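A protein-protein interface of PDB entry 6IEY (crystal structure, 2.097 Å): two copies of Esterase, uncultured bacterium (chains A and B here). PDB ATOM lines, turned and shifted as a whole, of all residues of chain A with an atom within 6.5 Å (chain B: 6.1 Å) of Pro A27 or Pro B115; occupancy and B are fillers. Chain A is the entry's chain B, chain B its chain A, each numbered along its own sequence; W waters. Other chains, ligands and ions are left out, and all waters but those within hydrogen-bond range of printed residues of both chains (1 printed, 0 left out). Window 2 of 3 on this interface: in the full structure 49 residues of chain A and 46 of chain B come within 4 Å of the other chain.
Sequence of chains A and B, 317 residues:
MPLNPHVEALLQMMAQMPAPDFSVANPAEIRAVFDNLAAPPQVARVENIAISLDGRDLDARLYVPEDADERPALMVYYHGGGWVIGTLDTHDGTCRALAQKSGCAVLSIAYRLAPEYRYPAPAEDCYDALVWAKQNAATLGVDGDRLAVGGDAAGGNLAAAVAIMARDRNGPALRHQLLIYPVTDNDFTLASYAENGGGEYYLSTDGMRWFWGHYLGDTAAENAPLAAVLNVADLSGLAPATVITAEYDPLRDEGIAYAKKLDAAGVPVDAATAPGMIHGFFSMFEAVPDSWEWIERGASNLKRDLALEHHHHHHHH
O of Ala A25 lies within hydrogen-bond range of NE1 of Trp B210, 3.0 Å away. The backbone carbonyl oxygen (O) of Val B84 is in hydrogen-bond range of the guanidinium group (NE) of Arg A31 (2.7 Å). The guanidinium group (NH2) of Arg A31 sits at hydrogen-bond distance from the backbone carbonyl oxygen (O) of Ala B114 (2.9 Å). The guanidinium group (NH2) of Arg A31 is in salt-bridge range of the side-chain carboxylate (OE1) of Glu B116, 2.8 Å away.
The backbone carbonyl oxygen (O) of Trp B83 lies within hydrogen-bond range of the backbone NH (N) of Ala B114 (2.8 Å). The backbone carbonyl oxygen (O) of His B214 lies within hydrogen-bond range of the guanidinium group (NH1) of Arg B118, 2.9 Å away.
CZ2 of Trp B210 touches C of Asn A26, 3.9 Å away. Pro B115 touches Pro A27 (CD to CG, 3.5 Å). CZ2 of Trp B210 touches N of Pro A27, at 3.9 Å. His B214 touches Pro A27. Ile B85 touches Ile A30. Ile A30 touches Trp B210. Arg A31 touches Ile B85 (CG to CG2, 3.6 Å). Leu B113 touches Arg A31.
Of the printed residues of chain B, Ala A25 touches Trp B210. Of the printed residues of chain B, Pro A27 touches Pro B115 (3.5 Å), Trp B210 (3.9 Å) and His B214 (3.9 Å). Of the printed residues of chain B, Ile A30 touches Ile B85 (3.8 Å) and Trp B210 (3.6 Å). Of the printed residues of chain A, Val B84 touches Arg A31 (2.7 Å). Pro B115 touches one residue of chain A. Printed residues of chain A within 4 Å of Glu B116: Arg A31. The nearest printed residue of chain B that does not touch Pro A27 is Val B84 (4.01 Å). The nearest residue of chain A that does not touch Pro B115 is Arg A31 (4.1 Å).
Printed residues of chain B that touch a printed residue of chain A: Val B84, Ile B85, Leu B113, Ala B114, Pro B115, Glu B116, Trp B210 and His B214. Hydrophobic or aromatic side chains of chain B that line the printed part of chain A: Val B84, Ile B85, Leu B113, Pro B115, Trp B210 and His B214. Along chain A the printed residues that touch a printed residue of chain B span positions 25 to 31. Among the printed residues, 12 pairs touch across the chains. Among the printed residues, Asp or Glu carboxylates within 4 Å of a Lys or Arg side-chain nitrogen of the other chain: Arg A31 with Glu B116 (2.8 Å).
No position is printed for both chains.
Water W1 lies within hydrogen-bond range of a ring nitrogen (NE2) of His B214, the side-chain amide oxygen of Asn A26 and the backbone carbonyl oxygen of Ala A25.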
ATOM      1  N   ALA A  25      21.260  20.439 -19.884  1.00  0.00           N
ATOM      2  CA  ALA A  25      20.883  19.178 -20.490  1.00  0.00           C
ATOM      3  C   ALA A  25      20.260  18.223 -19.477  1.00  0.00           C
ATOM      4  O   ALA A  25      20.910  17.297 -18.988  1.00  0.00           O
ATOM      5  CB  ALA A  25      22.107  18.531 -21.138  1.00  0.00           C
ATOM      6  N   ASN A  26      19.000  18.446 -19.157  1.00  0.00           N
ATOM      7  CA  ASN A  26      18.256  17.491 -18.353  1.00  0.00           C
ATOM      8  C   ASN A  26      17.293  16.745 -19.265  1.00  0.00           C
ATOM      9  O   ASN A  26      16.997  17.224 -20.365  1.00  0.00           O
ATOM     10  CB  ASN A  26      17.543  18.197 -17.200  1.00  0.00           C
ATOM     11  CG  ASN A  26      18.439  18.332 -15.973  1.00  0.00           C
ATOM     12  OD1 ASN A  26      19.314  17.513 -15.765  1.00  0.00           O
ATOM     13  ND2 ASN A  26      18.227  19.371 -15.171  1.00  0.00           N
ATOM     14  N   PRO A  27      16.832  15.562 -18.832  1.00  0.00           N
ATOM     15  CA  PRO A  27      15.956  14.754 -19.687  1.00  0.00           C
ATOM     16  C   PRO A  27      14.779  15.536 -20.295  1.00  0.00           C
ATOM     17  O   PRO A  27      14.536  15.355 -21.486  1.00  0.00           O
ATOM     18  CB  PRO A  27      15.472  13.657 -18.735  1.00  0.00           C
ATOM     19  CG  PRO A  27      16.656  13.487 -17.757  1.00  0.00           C
ATOM     20  CD  PRO A  27      17.126  14.890 -17.547  1.00  0.00           C
ATOM     21  N   ALA A  28      14.093  16.401 -19.542  1.00  0.00           N
ATOM     22  CA  ALA A  28      12.945  17.127 -20.115  1.00  0.00           C
ATOM     23  C   ALA A  28      13.354  18.027 -21.299  1.00  0.00           C
ATOM     24  O   ALA A  28      12.671  18.061 -22.334  1.00  0.00           O
ATOM     25  CB  ALA A  28      12.245  17.956 -19.040  1.00  0.00           C
ATOM     26  N   GLU A  29      14.471  18.742 -21.150  1.00  0.00           N
ATOM     27  CA  GLU A  29      15.007  19.598 -22.213  1.00  0.00           C
ATOM     28  C   GLU A  29      15.419  18.819 -23.453  1.00  0.00           C
ATOM     29  O   GLU A  29      15.131  19.227 -24.577  1.00  0.00           O
ATOM     30  CB  GLU A  29      16.229  20.387 -21.725  1.00  0.00           C
ATOM     31  CG  GLU A  29      15.930  21.523 -20.776  1.00  0.00           C
ATOM     32  CD  GLU A  29      15.774  21.082 -19.327  1.00  0.00           C
ATOM     33  OE1 GLU A  29      15.506  19.881 -19.060  1.00  0.00           O
ATOM     34  OE2 GLU A  29      15.943  21.952 -18.450  1.00  0.00           O
ATOM     35  N   ILE A  30      16.154  17.733 -23.245  1.00  0.00           N
ATOM     36  CA  ILE A  30      16.651  16.943 -24.365  1.00  0.00           C
ATOM     37  C   ILE A  30      15.456  16.352 -25.113  1.00  0.00           C
ATOM     38  O   ILE A  30      15.409  16.385 -26.341  1.00  0.00           O
ATOM     39  CB  ILE A  30      17.616  15.842 -23.895  1.00  0.00           C
ATOM     40  CG1 ILE A  30      18.750  16.468 -23.080  1.00  0.00           C
ATOM     41  CG2 ILE A  30      18.207  15.098 -25.073  1.00  0.00           C
ATOM     42  CD1 ILE A  30      19.400  17.600 -23.785  1.00  0.00           C
ATOM     43  N   ARG A  31      14.478  15.848 -24.366  1.00  0.00           N
ATOM     44  CA  ARG A  31      13.250  15.315 -24.965  1.00  0.00           C
ATOM     45  C   ARG A  31      12.499  16.332 -25.821  1.00  0.00           C
ATOM     46  O   ARG A  31      12.044  16.003 -26.903  1.00  0.00           O
ATOM     47  CB  ARG A  31      12.327  14.777 -23.882  1.00  0.00           C
ATOM     48  CG  ARG A  31      12.812  13.468 -23.291  1.00  0.00           C
ATOM     49  CD  ARG A  31      12.091  13.132 -22.024  1.00  0.00           C
ATOM     50  NE  ARG A  31      12.605  11.897 -21.453  1.00  0.00           N
ATOM     51  CZ  ARG A  31      12.420  11.519 -20.194  1.00  0.00           C
ATOM     52  NH1 ARG A  31      11.747  12.292 -19.350  1.00  0.00           N
ATOM     53  NH2 ARG A  31      12.934  10.380 -19.770  1.00  0.00           N
ATOM     54  N   ALA A  32      12.380  17.569 -25.347  1.00  0.00           N
ATOM     55  CA  ALA A  32      11.690  18.616 -26.110  1.00  0.00           C
ATOM     56  C   ALA A  32      12.443  18.965 -27.389  1.00  0.00           C
ATOM     57  O   ALA A  32      11.845  19.278 -28.424  1.00  0.00           O
ATOM     58  CB  ALA A  32      11.506  19.866 -25.258  1.00  0.00           C
ATOM     59  N   TRP B  83      17.825   5.381 -24.487  1.00  0.00           N
ATOM     60  CA  TRP B  83      16.995   4.917 -23.355  1.00  0.00           C
ATOM     61  C   TRP B  83      16.340   6.066 -22.553  1.00  0.00           C
ATOM     62  O   TRP B  83      15.723   5.841 -21.503  1.00  0.00           O
ATOM     63  CB  TRP B  83      17.803   4.063 -22.369  1.00  0.00           C
ATOM     64  CG  TRP B  83      18.635   2.927 -22.952  1.00  0.00           C
ATOM     65  CD1 TRP B  83      18.188   1.702 -23.386  1.00  0.00           C
ATOM     66  CD2 TRP B  83      20.060   2.904 -23.079  1.00  0.00           C
ATOM     67  NE1 TRP B  83      19.253   0.936 -23.813  1.00  0.00           N
ATOM     68  CE2 TRP B  83      20.411   1.650 -23.635  1.00  0.00           C
ATOM     69  CE3 TRP B  83      21.072   3.830 -22.798  1.00  0.00           C
ATOM     70  CZ2 TRP B  83      21.744   1.293 -23.900  1.00  0.00           C
ATOM     71  CZ3 TRP B  83      22.401   3.482 -23.071  1.00  0.00           C
ATOM     72  CH2 TRP B  83      22.723   2.220 -23.616  1.00  0.00           C
ATOM     73  N   VAL B  84      16.494   7.292 -23.026  1.00  0.00           N
ATOM     74  CA  VAL B  84      16.014   8.452 -22.264  1.00  0.00           C
ATOM     75  C   VAL B  84      15.006   9.255 -23.067  1.00  0.00           C
ATOM     76  O   VAL B  84      14.105   9.851 -22.505  1.00  0.00           O
ATOM     77  CB  VAL B  84      17.200   9.400 -21.838  1.00  0.00           C
ATOM     78  CG1 VAL B  84      16.700  10.634 -21.071  1.00  0.00           C
ATOM     79  CG2 VAL B  84      18.201   8.654 -20.993  1.00  0.00           C
ATOM     80  N   ILE B  85      15.164   9.283 -24.389  1.00  0.00           N
ATOM     81  CA  ILE B  85      14.323  10.137 -25.206  1.00  0.00           C
ATOM     82  C   ILE B  85      13.712   9.339 -26.345  1.00  0.00           C
ATOM     83  O   ILE B  85      14.001   8.157 -26.525  1.00  0.00           O
ATOM     84  CB  ILE B  85      15.113  11.364 -25.769  1.00  0.00           C
ATOM     85  CG1 ILE B  85      16.127  10.935 -26.831  1.00  0.00           C
ATOM     86  CG2 ILE B  85      15.830  12.115 -24.651  1.00  0.00           C
ATOM     87  CD1 ILE B  85      16.983  12.096 -27.408  1.00  0.00           C
ATOM     88  N   LEU B 113      10.987   5.141 -19.933  1.00  0.00           N
ATOM     89  CA  LEU B 113      12.253   5.782 -20.215  1.00  0.00           C
ATOM     90  C   LEU B 113      13.043   6.091 -18.956  1.00  0.00           C
ATOM     91  O   LEU B 113      12.489   6.443 -17.902  1.00  0.00           O
ATOM     92  CB  LEU B 113      12.024   7.078 -21.018  1.00  0.00           C
ATOM     93  CG  LEU B 113      11.378   7.019 -22.413  1.00  0.00           C
ATOM     94  CD1 LEU B 113      11.361   8.393 -23.055  1.00  0.00           C
ATOM     95  CD2 LEU B 113      12.102   6.036 -23.314  1.00  0.00           C
ATOM     96  N   ALA B 114      14.361   5.955 -19.085  1.00  0.00           N
ATOM     97  CA  ALA B 114      15.305   6.427 -18.086  1.00  0.00           C
ATOM     98  C   ALA B 114      15.401   7.965 -18.121  1.00  0.00           C
ATOM     99  O   ALA B 114      15.174   8.577 -19.156  1.00  0.00           O
ATOM    100  CB  ALA B 114      16.680   5.775 -18.337  1.00  0.00           C
ATOM    101  N   PRO B 115      15.774   8.611 -17.000  1.00  0.00           N
ATOM    102  CA  PRO B 115      16.149   8.085 -15.684  1.00  0.00           C
ATOM    103  C   PRO B 115      14.968   7.770 -14.778  1.00  0.00           C
ATOM    104  O   PRO B 115      15.193   7.205 -13.711  1.00  0.00           O
ATOM    105  CB  PRO B 115      16.995   9.218 -15.082  1.00  0.00           C
ATOM    106  CG  PRO B 115      16.486  10.436 -15.717  1.00  0.00           C
ATOM    107  CD  PRO B 115      16.082  10.044 -17.122  1.00  0.00           C
ATOM    108  N   GLU B 116      13.747   8.118 -15.181  1.00  0.00           N
ATOM    109  CA  GLU B 116      12.588   7.789 -14.364  1.00  0.00           C
ATOM    110  C   GLU B 116      12.543   6.304 -14.112  1.00  0.00           C
ATOM    111  O   GLU B 116      12.318   5.868 -12.986  1.00  0.00           O
ATOM    112  CB  GLU B 116      11.286   8.239 -15.026  1.00  0.00           C
ATOM    113  CG  GLU B 116      11.081   9.743 -15.104  1.00  0.00           C
ATOM    114  CD  GLU B 116      11.761  10.376 -16.305  1.00  0.00           C
ATOM    115  OE1 GLU B 116      12.427   9.655 -17.083  1.00  0.00           O
ATOM    116  OE2 GLU B 116      11.631  11.602 -16.483  1.00  0.00           O
ATOM    117  N   TYR B 117      12.733   5.525 -15.172  1.00  0.00           N
ATOM    118  CA  TYR B 117      12.814   4.071 -15.063  1.00  0.00           C
ATOM    119  C   TYR B 117      14.199   3.607 -15.525  1.00  0.00           C
ATOM    120  O   TYR B 117      14.508   3.584 -16.722  1.00  0.00           O
ATOM    121  CB  TYR B 117      11.681   3.409 -15.875  1.00  0.00           C
ATOM    122  CG  TYR B 117      10.344   3.857 -15.356  1.00  0.00           C
ATOM    123  CD1 TYR B 117       9.732   3.190 -14.315  1.00  0.00           C
ATOM    124  CD2 TYR B 117       9.734   4.998 -15.857  1.00  0.00           C
ATOM    125  CE1 TYR B 117       8.533   3.623 -13.801  1.00  0.00           C
ATOM    126  CE2 TYR B 117       8.541   5.440 -15.356  1.00  0.00           C
ATOM    127  CZ  TYR B 117       7.939   4.750 -14.323  1.00  0.00           C
ATOM    128  OH  TYR B 117       6.737   5.184 -13.814  1.00  0.00           O
ATOM    129  N   ARG B 118      15.042   3.260 -14.564  1.00  0.00           N
ATOM    130  CA  ARG B 118      16.398   2.844 -14.883  1.00  0.00           C
ATOM    131  C   ARG B 118      16.462   1.364 -15.267  1.00  0.00           C
ATOM    132  O   ARG B 118      15.507   0.611 -15.033  1.00  0.00           O
ATOM    133  CB  ARG B 118      17.317   3.143 -13.701  1.00  0.00           C
ATOM    134  CG  ARG B 118      17.428   4.627 -13.426  1.00  0.00           C
ATOM    135  CD  ARG B 118      18.437   4.923 -12.360  1.00  0.00           C
ATOM    136  NE  ARG B 118      18.280   6.277 -11.837  1.00  0.00           N
ATOM    137  CZ  ARG B 118      18.914   7.330 -12.325  1.00  0.00           C
ATOM    138  NH1 ARG B 118      19.744   7.181 -13.339  1.00  0.00           N
ATOM    139  NH2 ARG B 118      18.732   8.528 -11.792  1.00  0.00           N
ATOM    140  N   TRP B 210      26.241  10.567 -20.973  1.00  0.00           N
ATOM    141  CA  TRP B 210      24.969  11.073 -20.469  1.00  0.00           C
ATOM    142  C   TRP B 210      23.873   9.992 -20.472  1.00  0.00           C
ATOM    143  O   TRP B 210      23.255   9.701 -19.442  1.00  0.00           O
ATOM    144  CB  TRP B 210      24.570  12.267 -21.332  1.00  0.00           C
ATOM    145  CG  TRP B 210      23.486  13.117 -20.798  1.00  0.00           C
ATOM    146  CD1 TRP B 210      23.612  14.168 -19.934  1.00  0.00           C
ATOM    147  CD2 TRP B 210      22.101  13.025 -21.127  1.00  0.00           C
ATOM    148  NE1 TRP B 210      22.377  14.729 -19.692  1.00  0.00           N
ATOM    149  CE2 TRP B 210      21.434  14.050 -20.419  1.00  0.00           C
ATOM    150  CE3 TRP B 210      21.355  12.181 -21.963  1.00  0.00           C
ATOM    151  CZ2 TRP B 210      20.053  14.244 -20.513  1.00  0.00           C
ATOM    152  CZ3 TRP B 210      19.981  12.382 -22.050  1.00  0.00           C
ATOM    153  CH2 TRP B 210      19.349  13.402 -21.332  1.00  0.00           C
ATOM    154  N   HIS B 214      22.269   8.078 -17.212  1.00  0.00           N
ATOM    155  CA  HIS B 214      20.852   8.038 -16.948  1.00  0.00           C
ATOM    156  C   HIS B 214      20.286   6.627 -16.935  1.00  0.00           C
ATOM    157  O   HIS B 214      19.485   6.295 -16.066  1.00  0.00           O
ATOM    158  CB  HIS B 214      20.136   8.911 -17.968  1.00  0.00           C
ATOM    159  CG  HIS B 214      20.205  10.365 -17.631  1.00  0.00           C
ATOM    160  ND1 HIS B 214      20.007  10.832 -16.348  1.00  0.00           N
ATOM    161  CD2 HIS B 214      20.483  11.451 -18.391  1.00  0.00           C
ATOM    162  CE1 HIS B 214      20.141  12.148 -16.335  1.00  0.00           C
ATOM    163  NE2 HIS B 214      20.430  12.549 -17.561  1.00  0.00           N
ATOM    164  N   TYR B 215      20.720   5.778 -17.863  1.00  0.00           N
ATOM    165  CA  TYR B 215      20.160   4.429 -17.960  1.00  0.00           C
ATOM    166  C   TYR B 215      20.541   3.555 -16.772  1.00  0.00           C
ATOM    167  O   TYR B 215      19.675   2.913 -16.158  1.00  0.00           O
ATOM    168  CB  TYR B 215      20.622   3.749 -19.271  1.00  0.00           C
ATOM    169  CG  TYR B 215      19.913   2.455 -19.584  1.00  0.00           C
ATOM    170  CD1 TYR B 215      18.598   2.234 -19.179  1.00  0.00           C
ATOM    171  CD2 TYR B 215      20.558   1.447 -20.299  1.00  0.00           C
ATOM    172  CE1 TYR B 215      17.948   1.031 -19.487  1.00  0.00           C
ATOM    173  CE2 TYR B 215      19.929   0.258 -20.602  1.00  0.00           C
ATOM    174  CZ  TYR B 215      18.627   0.052 -20.201  1.00  0.00           C
ATOM    175  OH  TYR B 215      18.027  -1.144 -20.529  1.00  0.00           O
HETATM  176  O   HOH W   1      20.728  15.040 -16.338  1.00  0.00           O
